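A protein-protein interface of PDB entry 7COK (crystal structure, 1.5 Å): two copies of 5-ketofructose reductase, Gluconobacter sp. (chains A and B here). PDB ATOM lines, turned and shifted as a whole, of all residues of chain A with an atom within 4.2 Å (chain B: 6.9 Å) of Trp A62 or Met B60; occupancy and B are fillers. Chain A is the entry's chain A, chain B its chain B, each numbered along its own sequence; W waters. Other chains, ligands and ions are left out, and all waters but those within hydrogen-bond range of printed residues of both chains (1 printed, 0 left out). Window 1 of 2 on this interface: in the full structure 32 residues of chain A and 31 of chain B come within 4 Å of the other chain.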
ATOM      1  N   LEU A  10      -6.990  32.336  16.678  1.00  0.00           N
ATOM      2  CA  LEU A  10      -7.342  31.324  15.686  1.00  0.00           C
ATOM      3  C   LEU A  10      -6.103  30.671  15.120  1.00  0.00           C
ATOM      4  O   LEU A  10      -5.142  31.345  14.742  1.00  0.00           O
ATOM      5  CB  LEU A  10      -8.173  31.934  14.552  1.00  0.00           C
ATOM      6  CG  LEU A  10      -9.504  32.555  15.021  1.00  0.00           C
ATOM      7  CD1 LEU A  10     -10.175  33.272  13.861  1.00  0.00           C
ATOM      8  CD2 LEU A  10     -10.420  31.487  15.640  1.00  0.00           C
ATOM      9  N   THR A  11      -6.143  29.345  15.104  1.00  0.00           N
ATOM     10  CA  THR A  11      -5.171  28.468  14.482  1.00  0.00           C
ATOM     11  C   THR A  11      -5.994  27.380  13.784  1.00  0.00           C
ATOM     12  O   THR A  11      -7.226  27.334  13.945  1.00  0.00           O
ATOM     13  CB  THR A  11      -4.228  27.816  15.536  1.00  0.00           C
ATOM     14  OG1 THR A  11      -4.983  27.009  16.461  1.00  0.00           O
ATOM     15  CG2 THR A  11      -3.429  28.856  16.308  1.00  0.00           C
ATOM     16  N   GLY A  12      -5.351  26.509  12.997  1.00  0.00           N
ATOM     17  CA  GLY A  12      -6.078  25.373  12.453  1.00  0.00           C
ATOM     18  C   GLY A  12      -5.246  24.592  11.474  1.00  0.00           C
ATOM     19  O   GLY A  12      -4.015  24.611  11.561  1.00  0.00           O
ATOM     20  N   PHE A  14      -5.134  22.833   7.200  1.00  0.00           N
ATOM     21  CA  PHE A  14      -5.625  22.640   5.840  1.00  0.00           C
ATOM     22  C   PHE A  14      -5.145  21.266   5.392  1.00  0.00           C
ATOM     23  O   PHE A  14      -3.951  20.950   5.445  1.00  0.00           O
ATOM     24  CB  PHE A  14      -5.061  23.703   4.897  1.00  0.00           C
ATOM     25  CG  PHE A  14      -5.322  25.115   5.320  1.00  0.00           C
ATOM     26  CD1 PHE A  14      -6.533  25.495   5.960  1.00  0.00           C
ATOM     27  CD2 PHE A  14      -4.379  26.119   5.026  1.00  0.00           C
ATOM     28  CE1 PHE A  14      -6.759  26.823   6.321  1.00  0.00           C
ATOM     29  CE2 PHE A  14      -4.615  27.450   5.397  1.00  0.00           C
ATOM     30  CZ  PHE A  14      -5.790  27.806   6.035  1.00  0.00           C
ATOM     31  N   ILE A  41      -9.026  25.190  14.067  1.00  0.00           N
ATOM     32  CA  ILE A  41     -10.051  24.977  13.065  1.00  0.00           C
ATOM     33  C   ILE A  41      -9.576  23.983  11.992  1.00  0.00           C
ATOM     34  O   ILE A  41      -8.724  24.311  11.159  1.00  0.00           O
ATOM     35  CB  ILE A  41     -10.499  26.328  12.422  1.00  0.00           C
ATOM     36  CG1 ILE A  41     -10.815  27.414  13.494  1.00  0.00           C
ATOM     37  CG2 ILE A  41     -11.651  26.107  11.459  1.00  0.00           C
ATOM     38  CD1 ILE A  41     -11.762  27.022  14.610  1.00  0.00           C
ATOM     39  N   CYS A  43      -9.909  22.245   8.754  1.00  0.00           N
ATOM     40  CA  CYS A  43     -10.571  22.550   7.471  1.00  0.00           C
ATOM     41  C   CYS A  43     -10.244  21.541   6.391  1.00  0.00           C
ATOM     42  O   CYS A  43      -9.102  21.131   6.243  1.00  0.00           O
ATOM     43  CB  CYS A  43     -10.129  23.915   6.961  1.00  0.00           C
ATOM     44  SG  CYS A  43     -10.443  25.288   8.089  1.00  0.00           S
ATOM     45  N   ALA A  53      -7.142  29.487   0.759  1.00  0.00           N
ATOM     46  CA  ALA A  53      -7.203  29.184   2.180  1.00  0.00           C
ATOM     47  C   ALA A  53      -6.081  29.864   2.932  1.00  0.00           C
ATOM     48  O   ALA A  53      -6.299  30.379   4.037  1.00  0.00           O
ATOM     49  CB  ALA A  53      -7.182  27.677   2.436  1.00  0.00           C
ATOM     50  N   GLY A  56      -6.775  33.343   3.089  1.00  0.00           N
ATOM     51  CA  GLY A  56      -7.938  33.444   3.986  1.00  0.00           C
ATOM     52  C   GLY A  56      -7.548  33.472   5.454  1.00  0.00           C
ATOM     53  O   GLY A  56      -8.024  34.318   6.196  1.00  0.00           O
ATOM     54  N   ALA A  57      -6.647  32.572   5.858  1.00  0.00           N
ATOM     55  CA  ALA A  57      -6.174  32.604   7.237  1.00  0.00           C
ATOM     56  C   ALA A  57      -5.473  33.920   7.569  1.00  0.00           C
ATOM     57  O   ALA A  57      -5.614  34.449   8.651  1.00  0.00           O
ATOM     58  CB  ALA A  57      -5.273  31.433   7.521  1.00  0.00           C
ATOM     59  N   MET A  60      -8.274  36.588   7.939  1.00  0.00           N
ATOM     60  CA  MET A  60      -9.042  36.306   9.150  1.00  0.00           C
ATOM     61  C   MET A  60      -8.172  36.439  10.372  1.00  0.00           C
ATOM     62  O   MET A  60      -8.648  36.192  11.486  1.00  0.00           O
ATOM     63  CB  MET A  60      -9.651  34.908   9.127  1.00  0.00           C
ATOM     64  CG  MET A  60     -10.669  34.647   8.051  1.00  0.00           C
ATOM     65  SD  MET A  60     -11.066  32.901   7.973  1.00  0.00           S
ATOM     66  CE  MET A  60     -11.980  32.829   6.437  1.00  0.00           C
ATOM     67  N   GLU A  61      -6.889  36.779  10.171  1.00  0.00           N
ATOM     68  CA  GLU A  61      -5.951  37.082  11.267  1.00  0.00           C
ATOM     69  C   GLU A  61      -5.680  35.885  12.197  1.00  0.00           C
ATOM     70  O   GLU A  61      -5.455  36.034  13.401  1.00  0.00           O
ATOM     71  CB  GLU A  61      -6.377  38.357  12.030  1.00  0.00           C
ATOM     72  CG  GLU A  61      -6.514  39.533  11.046  1.00  0.00           C
ATOM     73  CD  GLU A  61      -6.519  40.922  11.656  1.00  0.00           C
ATOM     74  OE1 GLU A  61      -6.436  41.063  12.893  1.00  0.00           O
ATOM     75  OE2 GLU A  61      -6.591  41.888  10.855  1.00  0.00           O
ATOM     76  N   TRP A  62      -5.678  34.684  11.628  1.00  0.00           N
ATOM     77  CA  TRP A  62      -5.077  33.544  12.307  1.00  0.00           C
ATOM     78  C   TRP A  62      -3.610  33.797  12.660  1.00  0.00           C
ATOM     79  O   TRP A  62      -2.937  34.614  12.006  1.00  0.00           O
ATOM     80  CB  TRP A  62      -5.157  32.317  11.412  1.00  0.00           C
ATOM     81  CG  TRP A  62      -6.553  31.791  11.066  1.00  0.00           C
ATOM     82  CD1 TRP A  62      -7.734  32.494  11.017  1.00  0.00           C
ATOM     83  CD2 TRP A  62      -6.859  30.466  10.639  1.00  0.00           C
ATOM     84  NE1 TRP A  62      -8.769  31.671  10.635  1.00  0.00           N
ATOM     85  CE2 TRP A  62      -8.265  30.430  10.366  1.00  0.00           C
ATOM     86  CE3 TRP A  62      -6.094  29.291  10.462  1.00  0.00           C
ATOM     87  CZ2 TRP A  62      -8.927  29.260   9.921  1.00  0.00           C
ATOM     88  CZ3 TRP A  62      -6.752  28.122  10.023  1.00  0.00           C
ATOM     89  CH2 TRP A  62      -8.161  28.122   9.754  1.00  0.00           C
ATOM     90  N   VAL A  63      -3.104  33.081  13.651  1.00  0.00           N
ATOM     91  CA  VAL A  63      -1.694  33.206  14.029  1.00  0.00           C
ATOM     92  C   VAL A  63      -0.838  32.073  13.495  1.00  0.00           C
ATOM     93  O   VAL A  63       0.397  32.126  13.544  1.00  0.00           O
ATOM     94  CB  VAL A  63      -1.484  33.392  15.551  1.00  0.00           C
ATOM     95  CG1 VAL A  63      -2.265  34.616  16.039  1.00  0.00           C
ATOM     96  CG2 VAL A  63      -1.910  32.148  16.294  1.00  0.00           C
ATOM     97  N   GLY A  64      -1.493  31.038  12.984  1.00  0.00           N
ATOM     98  CA  GLY A  64      -0.795  29.889  12.445  1.00  0.00           C
ATOM     99  C   GLY A  64      -1.736  28.846  11.921  1.00  0.00           C
ATOM    100  O   GLY A  64      -2.929  28.882  12.207  1.00  0.00           O
ATOM    101  N   PHE A  65      -1.179  27.920  11.143  1.00  0.00           N
ATOM    102  CA  PHE A  65      -1.934  26.757  10.700  1.00  0.00           C
ATOM    103  C   PHE A  65      -0.996  25.626  10.331  1.00  0.00           C
ATOM    104  O   PHE A  65       0.150  25.878  10.020  1.00  0.00           O
ATOM    105  CB  PHE A  65      -2.860  27.099   9.516  1.00  0.00           C
ATOM    106  CG  PHE A  65      -2.155  27.657   8.303  1.00  0.00           C
ATOM    107  CD1 PHE A  65      -1.674  26.803   7.290  1.00  0.00           C
ATOM    108  CD2 PHE A  65      -2.004  29.041   8.152  1.00  0.00           C
ATOM    109  CE1 PHE A  65      -1.042  27.338   6.149  1.00  0.00           C
ATOM    110  CE2 PHE A  65      -1.396  29.575   6.998  1.00  0.00           C
ATOM    111  CZ  PHE A  65      -0.907  28.725   6.008  1.00  0.00           C
ATOM    112  N   ILE A  97       1.985  32.879  11.158  1.00  0.00           N
ATOM    113  CA  ILE A  97       1.594  34.161  10.604  1.00  0.00           C
ATOM    114  C   ILE A  97       2.023  35.234  11.609  1.00  0.00           C
ATOM    115  O   ILE A  97       1.491  35.322  12.727  1.00  0.00           O
ATOM    116  CB  ILE A  97       0.084  34.269  10.258  1.00  0.00           C
ATOM    117  CG1 ILE A  97      -0.390  33.026   9.477  1.00  0.00           C
ATOM    118  CG2 ILE A  97      -0.188  35.558   9.484  1.00  0.00           C
ATOM    119  CD1 ILE A  97      -1.861  33.015   9.079  1.00  0.00           C
ATOM    120  N   ARG B   7     -14.036  16.770  11.700  1.00  0.00           N
ATOM    121  CA  ARG B   7     -14.418  17.904  10.891  1.00  0.00           C
ATOM    122  C   ARG B   7     -15.768  18.389  11.366  1.00  0.00           C
ATOM    123  O   ARG B   7     -16.751  17.647  11.335  1.00  0.00           O
ATOM    124  CB  ARG B   7     -14.456  17.548   9.418  1.00  0.00           C
ATOM    125  CG  ARG B   7     -14.889  18.699   8.521  1.00  0.00           C
ATOM    126  CD  ARG B   7     -15.290  18.197   7.153  1.00  0.00           C
ATOM    127  NE  ARG B   7     -15.388  19.316   6.221  1.00  0.00           N
ATOM    128  CZ  ARG B   7     -15.583  19.219   4.900  1.00  0.00           C
ATOM    129  NH1 ARG B   7     -15.716  18.046   4.284  1.00  0.00           N
ATOM    130  NH2 ARG B   7     -15.644  20.325   4.170  1.00  0.00           N
ATOM    131  N   SER B   8     -15.782  19.627  11.851  1.00  0.00           N
ATOM    132  CA  SER B   8     -17.006  20.325  12.209  1.00  0.00           C
ATOM    133  C   SER B   8     -17.497  21.129  11.017  1.00  0.00           C
ATOM    134  O   SER B   8     -16.691  21.646  10.246  1.00  0.00           O
ATOM    135  CB  SER B   8     -16.736  21.308  13.349  1.00  0.00           C
ATOM    136  OG  SER B   8     -16.206  20.673  14.506  1.00  0.00           O
ATOM    137  N   LEU B  10     -18.479  24.424   9.418  1.00  0.00           N
ATOM    138  CA  LEU B  10     -17.889  25.725   9.713  1.00  0.00           C
ATOM    139  C   LEU B  10     -18.804  26.885   9.327  1.00  0.00           C
ATOM    140  O   LEU B  10     -19.304  26.949   8.208  1.00  0.00           O
ATOM    141  CB  LEU B  10     -16.504  25.897   9.067  1.00  0.00           C
ATOM    142  CG  LEU B  10     -15.460  24.886   9.566  1.00  0.00           C
ATOM    143  CD1 LEU B  10     -14.164  25.167   8.827  1.00  0.00           C
ATOM    144  CD2 LEU B  10     -15.248  24.938  11.081  1.00  0.00           C
ATOM    145  N   ILE B  41     -17.001  30.770  13.906  1.00  0.00           N
ATOM    146  CA  ILE B  41     -15.686  31.408  14.013  1.00  0.00           C
ATOM    147  C   ILE B  41     -15.771  32.947  13.924  1.00  0.00           C
ATOM    148  O   ILE B  41     -16.058  33.505  12.856  1.00  0.00           O
ATOM    149  CB  ILE B  41     -14.742  30.861  12.917  1.00  0.00           C
ATOM    150  CG1 ILE B  41     -14.767  29.322  12.843  1.00  0.00           C
ATOM    151  CG2 ILE B  41     -13.338  31.405  13.143  1.00  0.00           C
ATOM    152  CD1 ILE B  41     -14.609  28.588  14.159  1.00  0.00           C
ATOM    153  N   CYS B  43     -14.190  36.252  13.457  1.00  0.00           N
ATOM    154  CA  CYS B  43     -12.927  36.789  12.926  1.00  0.00           C
ATOM    155  C   CYS B  43     -12.922  38.309  12.847  1.00  0.00           C
ATOM    156  O   CYS B  43     -13.891  38.928  12.412  1.00  0.00           O
ATOM    157  CB  CYS B  43     -12.674  36.273  11.514  1.00  0.00           C
ATOM    158  SG  CYS B  43     -12.794  34.491  11.278  1.00  0.00           S
ATOM    159  N   ASP B  52     -10.372  38.616   0.542  1.00  0.00           N
ATOM    160  CA  ASP B  52      -9.609  37.405   0.859  1.00  0.00           C
ATOM    161  C   ASP B  52     -10.273  36.555   1.963  1.00  0.00           C
ATOM    162  O   ASP B  52     -10.200  35.341   1.927  1.00  0.00           O
ATOM    163  CB  ASP B  52      -8.178  37.768   1.243  1.00  0.00           C
ATOM    164  CG  ASP B  52      -7.318  38.100   0.049  1.00  0.00           C
ATOM    165  OD1 ASP B  52      -7.793  38.006  -1.106  1.00  0.00           O
ATOM    166  OD2 ASP B  52      -6.166  38.473   0.294  1.00  0.00           O
ATOM    167  N   ALA B  53     -10.991  37.188   2.891  1.00  0.00           N
ATOM    168  CA  ALA B  53     -11.705  36.407   3.922  1.00  0.00           C
ATOM    169  C   ALA B  53     -12.878  35.633   3.310  1.00  0.00           C
ATOM    170  O   ALA B  53     -13.107  34.461   3.616  1.00  0.00           O
ATOM    171  CB  ALA B  53     -12.151  37.315   5.067  1.00  0.00           C
ATOM    172  N   LYS B  55     -13.104  34.635   0.073  1.00  0.00           N
ATOM    173  CA  LYS B  55     -12.493  33.568  -0.704  1.00  0.00           C
ATOM    174  C   LYS B  55     -11.958  32.461   0.215  1.00  0.00           C
ATOM    175  O   LYS B  55     -12.026  31.291  -0.134  1.00  0.00           O
ATOM    176  CB  LYS B  55     -11.335  34.079  -1.562  1.00  0.00           C
ATOM    177  CG  LYS B  55     -11.729  34.865  -2.804  1.00  0.00           C
ATOM    178  CD  LYS B  55     -10.478  35.561  -3.300  1.00  0.00           C
ATOM    179  CE  LYS B  55     -10.727  36.534  -4.425  1.00  0.00           C
ATOM    180  NZ  LYS B  55      -9.461  37.279  -4.715  1.00  0.00           N
ATOM    181  N   GLY B  56     -11.460  32.862   1.388  1.00  0.00           N
ATOM    182  CA  GLY B  56     -11.031  31.931   2.439  1.00  0.00           C
ATOM    183  C   GLY B  56     -12.154  31.031   2.944  1.00  0.00           C
ATOM    184  O   GLY B  56     -11.975  29.816   3.041  1.00  0.00           O
ATOM    185  N   ALA B  57     -13.306  31.635   3.260  1.00  0.00           N
ATOM    186  CA  ALA B  57     -14.464  30.843   3.730  1.00  0.00           C
ATOM    187  C   ALA B  57     -14.896  29.831   2.658  1.00  0.00           C
ATOM    188  O   ALA B  57     -15.171  28.682   2.985  1.00  0.00           O
ATOM    189  CB  ALA B  57     -15.600  31.752   4.149  1.00  0.00           C
ATOM    190  N   LYS B  58     -14.904  30.247   1.383  1.00  0.00           N
ATOM    191  CA  LYS B  58     -15.214  29.327   0.283  1.00  0.00           C
ATOM    192  C   LYS B  58     -14.192  28.176   0.225  1.00  0.00           C
ATOM    193  O   LYS B  58     -14.588  27.020   0.115  1.00  0.00           O
ATOM    194  CB  LYS B  58     -15.260  30.056  -1.063  1.00  0.00           C
ATOM    195  CG  LYS B  58     -16.495  30.919  -1.301  1.00  0.00           C
ATOM    196  CD  LYS B  58     -16.399  31.709  -2.610  1.00  0.00           C
ATOM    197  CE  LYS B  58     -16.689  30.857  -3.838  1.00  0.00           C
ATOM    198  NZ  LYS B  58     -16.558  31.583  -5.136  1.00  0.00           N
ATOM    199  N   ALA B  59     -12.894  28.496   0.302  1.00  0.00           N
ATOM    200  CA  ALA B  59     -11.822  27.486   0.180  1.00  0.00           C
ATOM    201  C   ALA B  59     -11.766  26.547   1.384  1.00  0.00           C
ATOM    202  O   ALA B  59     -11.340  25.394   1.259  1.00  0.00           O
ATOM    203  CB  ALA B  59     -10.468  28.171   0.003  1.00  0.00           C
ATOM    204  N   MET B  60     -12.169  27.060   2.546  1.00  0.00           N
ATOM    205  CA  MET B  60     -12.206  26.260   3.781  1.00  0.00           C
ATOM    206  C   MET B  60     -13.535  25.542   3.926  1.00  0.00           C
ATOM    207  O   MET B  60     -13.787  24.869   4.913  1.00  0.00           O
ATOM    208  CB  MET B  60     -11.967  27.147   4.993  1.00  0.00           C
ATOM    209  CG  MET B  60     -10.583  27.730   5.067  1.00  0.00           C
ATOM    210  SD  MET B  60     -10.515  28.829   6.486  1.00  0.00           S
ATOM    211  CE  MET B  60      -9.176  29.942   6.063  1.00  0.00           C
ATOM    212  N   GLU B  61     -14.402  25.719   2.932  1.00  0.00           N
ATOM    213  CA  GLU B  61     -15.692  25.008   2.835  1.00  0.00           C
ATOM    214  C   GLU B  61     -16.655  25.291   3.981  1.00  0.00           C
ATOM    215  O   GLU B  61     -17.411  24.426   4.402  1.00  0.00           O
ATOM    216  CB  GLU B  61     -15.524  23.509   2.541  1.00  0.00           C
ATOM    217  CG  GLU B  61     -14.595  23.293   1.352  1.00  0.00           C
ATOM    218  CD  GLU B  61     -14.472  21.866   0.875  1.00  0.00           C
ATOM    219  OE1 GLU B  61     -15.094  20.953   1.465  1.00  0.00           O
ATOM    220  OE2 GLU B  61     -13.717  21.682  -0.113  1.00  0.00           O
ATOM    221  N   TRP B  62     -16.659  26.536   4.448  1.00  0.00           N
ATOM    222  CA  TRP B  62     -17.738  27.009   5.318  1.00  0.00           C
ATOM    223  C   TRP B  62     -19.074  26.939   4.601  1.00  0.00           C
ATOM    224  O   TRP B  62     -19.133  26.977   3.361  1.00  0.00           O
ATOM    225  CB  TRP B  62     -17.509  28.447   5.757  1.00  0.00           C
ATOM    226  CG  TRP B  62     -16.271  28.755   6.556  1.00  0.00           C
ATOM    227  CD1 TRP B  62     -15.094  28.058   6.601  1.00  0.00           C
ATOM    228  CD2 TRP B  62     -16.084  29.927   7.354  1.00  0.00           C
ATOM    229  NE1 TRP B  62     -14.197  28.708   7.432  1.00  0.00           N
ATOM    230  CE2 TRP B  62     -14.783  29.865   7.885  1.00  0.00           C
ATOM    231  CE3 TRP B  62     -16.913  31.021   7.679  1.00  0.00           C
ATOM    232  CZ2 TRP B  62     -14.260  30.868   8.717  1.00  0.00           C
ATOM    233  CZ3 TRP B  62     -16.419  32.007   8.523  1.00  0.00           C
ATOM    234  CH2 TRP B  62     -15.102  31.917   9.052  1.00  0.00           C
ATOM    235  N   VAL B  63     -20.139  26.888   5.397  1.00  0.00           N
ATOM    236  CA  VAL B  63     -21.516  26.827   4.857  1.00  0.00           C
ATOM    237  C   VAL B  63     -22.233  28.170   4.911  1.00  0.00           C
ATOM    238  O   VAL B  63     -23.258  28.364   4.266  1.00  0.00           O
ATOM    239  CB  VAL B  63     -22.374  25.710   5.519  1.00  0.00           C
ATOM    240  CG1 VAL B  63     -21.745  24.340   5.304  1.00  0.00           C
ATOM    241  CG2 VAL B  63     -22.602  25.981   6.995  1.00  0.00           C
HETATM  242  O   HOH W   1      -8.404  34.177   0.261  1.00  0.00           O
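N of Val A63 lies within hydrogen-bond range of O of Leu A10 (2.9 Å).
O of Ile A41 sits at hydrogen-bond distance from SG of Cys A43, at 3.7 Å.
The backbone NH (N) of Trp A62 lies within hydrogen-bond range of the backbone carbonyl oxygen (O) of Ala A57.
O of Leu B10 lies within hydrogen-bond range of N of Val B63 (2.9 Å).
The backbone carbonyl oxygen of Ile B41 lies close to the side-chain sulfur of Cys B43, at 3.8 Å.
O of Ala B57 sits at hydrogen-bond distance from N of Trp B62 (3.0 Å).
Phe A14 touches Met B60 (CE1 to CE, 3.95 Å).
Ile B41 touches Ile A41 (CD1 to CD1, 3.3 Å).
SG of Cys A43 touches SD of Met B60 (3.9 Å).
Ala B59 touches Ala A53.
Asp B52 touches Gly A56.
Ala A57 touches Met B60 (N to CE, 3.7 Å).
Ala B53 touches Met A60.
CE of Met A60 touches C of Gly B56, at 3.9 Å.
Met A60 touches Met B60.
SD of Met B60 touches CZ2 of Trp A62 (3.8 Å).
Of the printed residues of chain B, Leu A10 touches Ile B41 and Cys B43.
Of the printed residues of chain B, Met A60 touches Cys B43, Ala B53, Gly B56, Ala B57, Met B60 and Trp B62.
Trp A62 touches one residue of chain B.
Printed residues of chain A within 4 Å of Leu B10: Ile A41 (3.8 Å) and Cys A43 (3.8 Å).
Of the printed residues of chain A, Asp B52 touches Gly A56 (3.6 Å).
Of the printed residues of chain A, Ala B53 touches Met A60 (3.4 Å).
Of the printed residues of chain A, Met B60 touches Phe A14 (3.95 Å), Cys A43 (3.9 Å), Ala A53 (3.5 Å), Gly A56 (3.9 Å), Ala A57 (3.7 Å), Met A60 (3.997 Å) and Trp A62 (3.8 Å).
The nearest residue of chain B that does not touch Trp A62 is Cys B43 (5.0 Å).
The nearest printed residue of chain B that does not touch Cys A43 is Trp B62 (5.1 Å).
Hydrophobic or aromatic side chains of chain A within 4 Å of the printed part of chain B: Leu A10, Phe A14, Ile A41, Met A60 and Trp A62.
Among the printed residues, no Asp or Glu carboxylate lies within 4 Å of a Lys or Arg side-chain nitrogen of the other chain.
Leu A10 touches Ile B41, and with the chains exchanged Ile A41 touches Leu B10.
Leu A10 touches Cys B43, and with the chains exchanged Cys A43 touches Leu B10.
Ala A53 touches Met B60, and with the chains exchanged Met A60 touches Ala B53.
Ala A57 touches Met B60, and with the chains exchanged Met A60 touches Ala B57.
Water W1 bridges O of Asp B52 (2.7 Å) and N of Gly A56 (3.4 Å).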
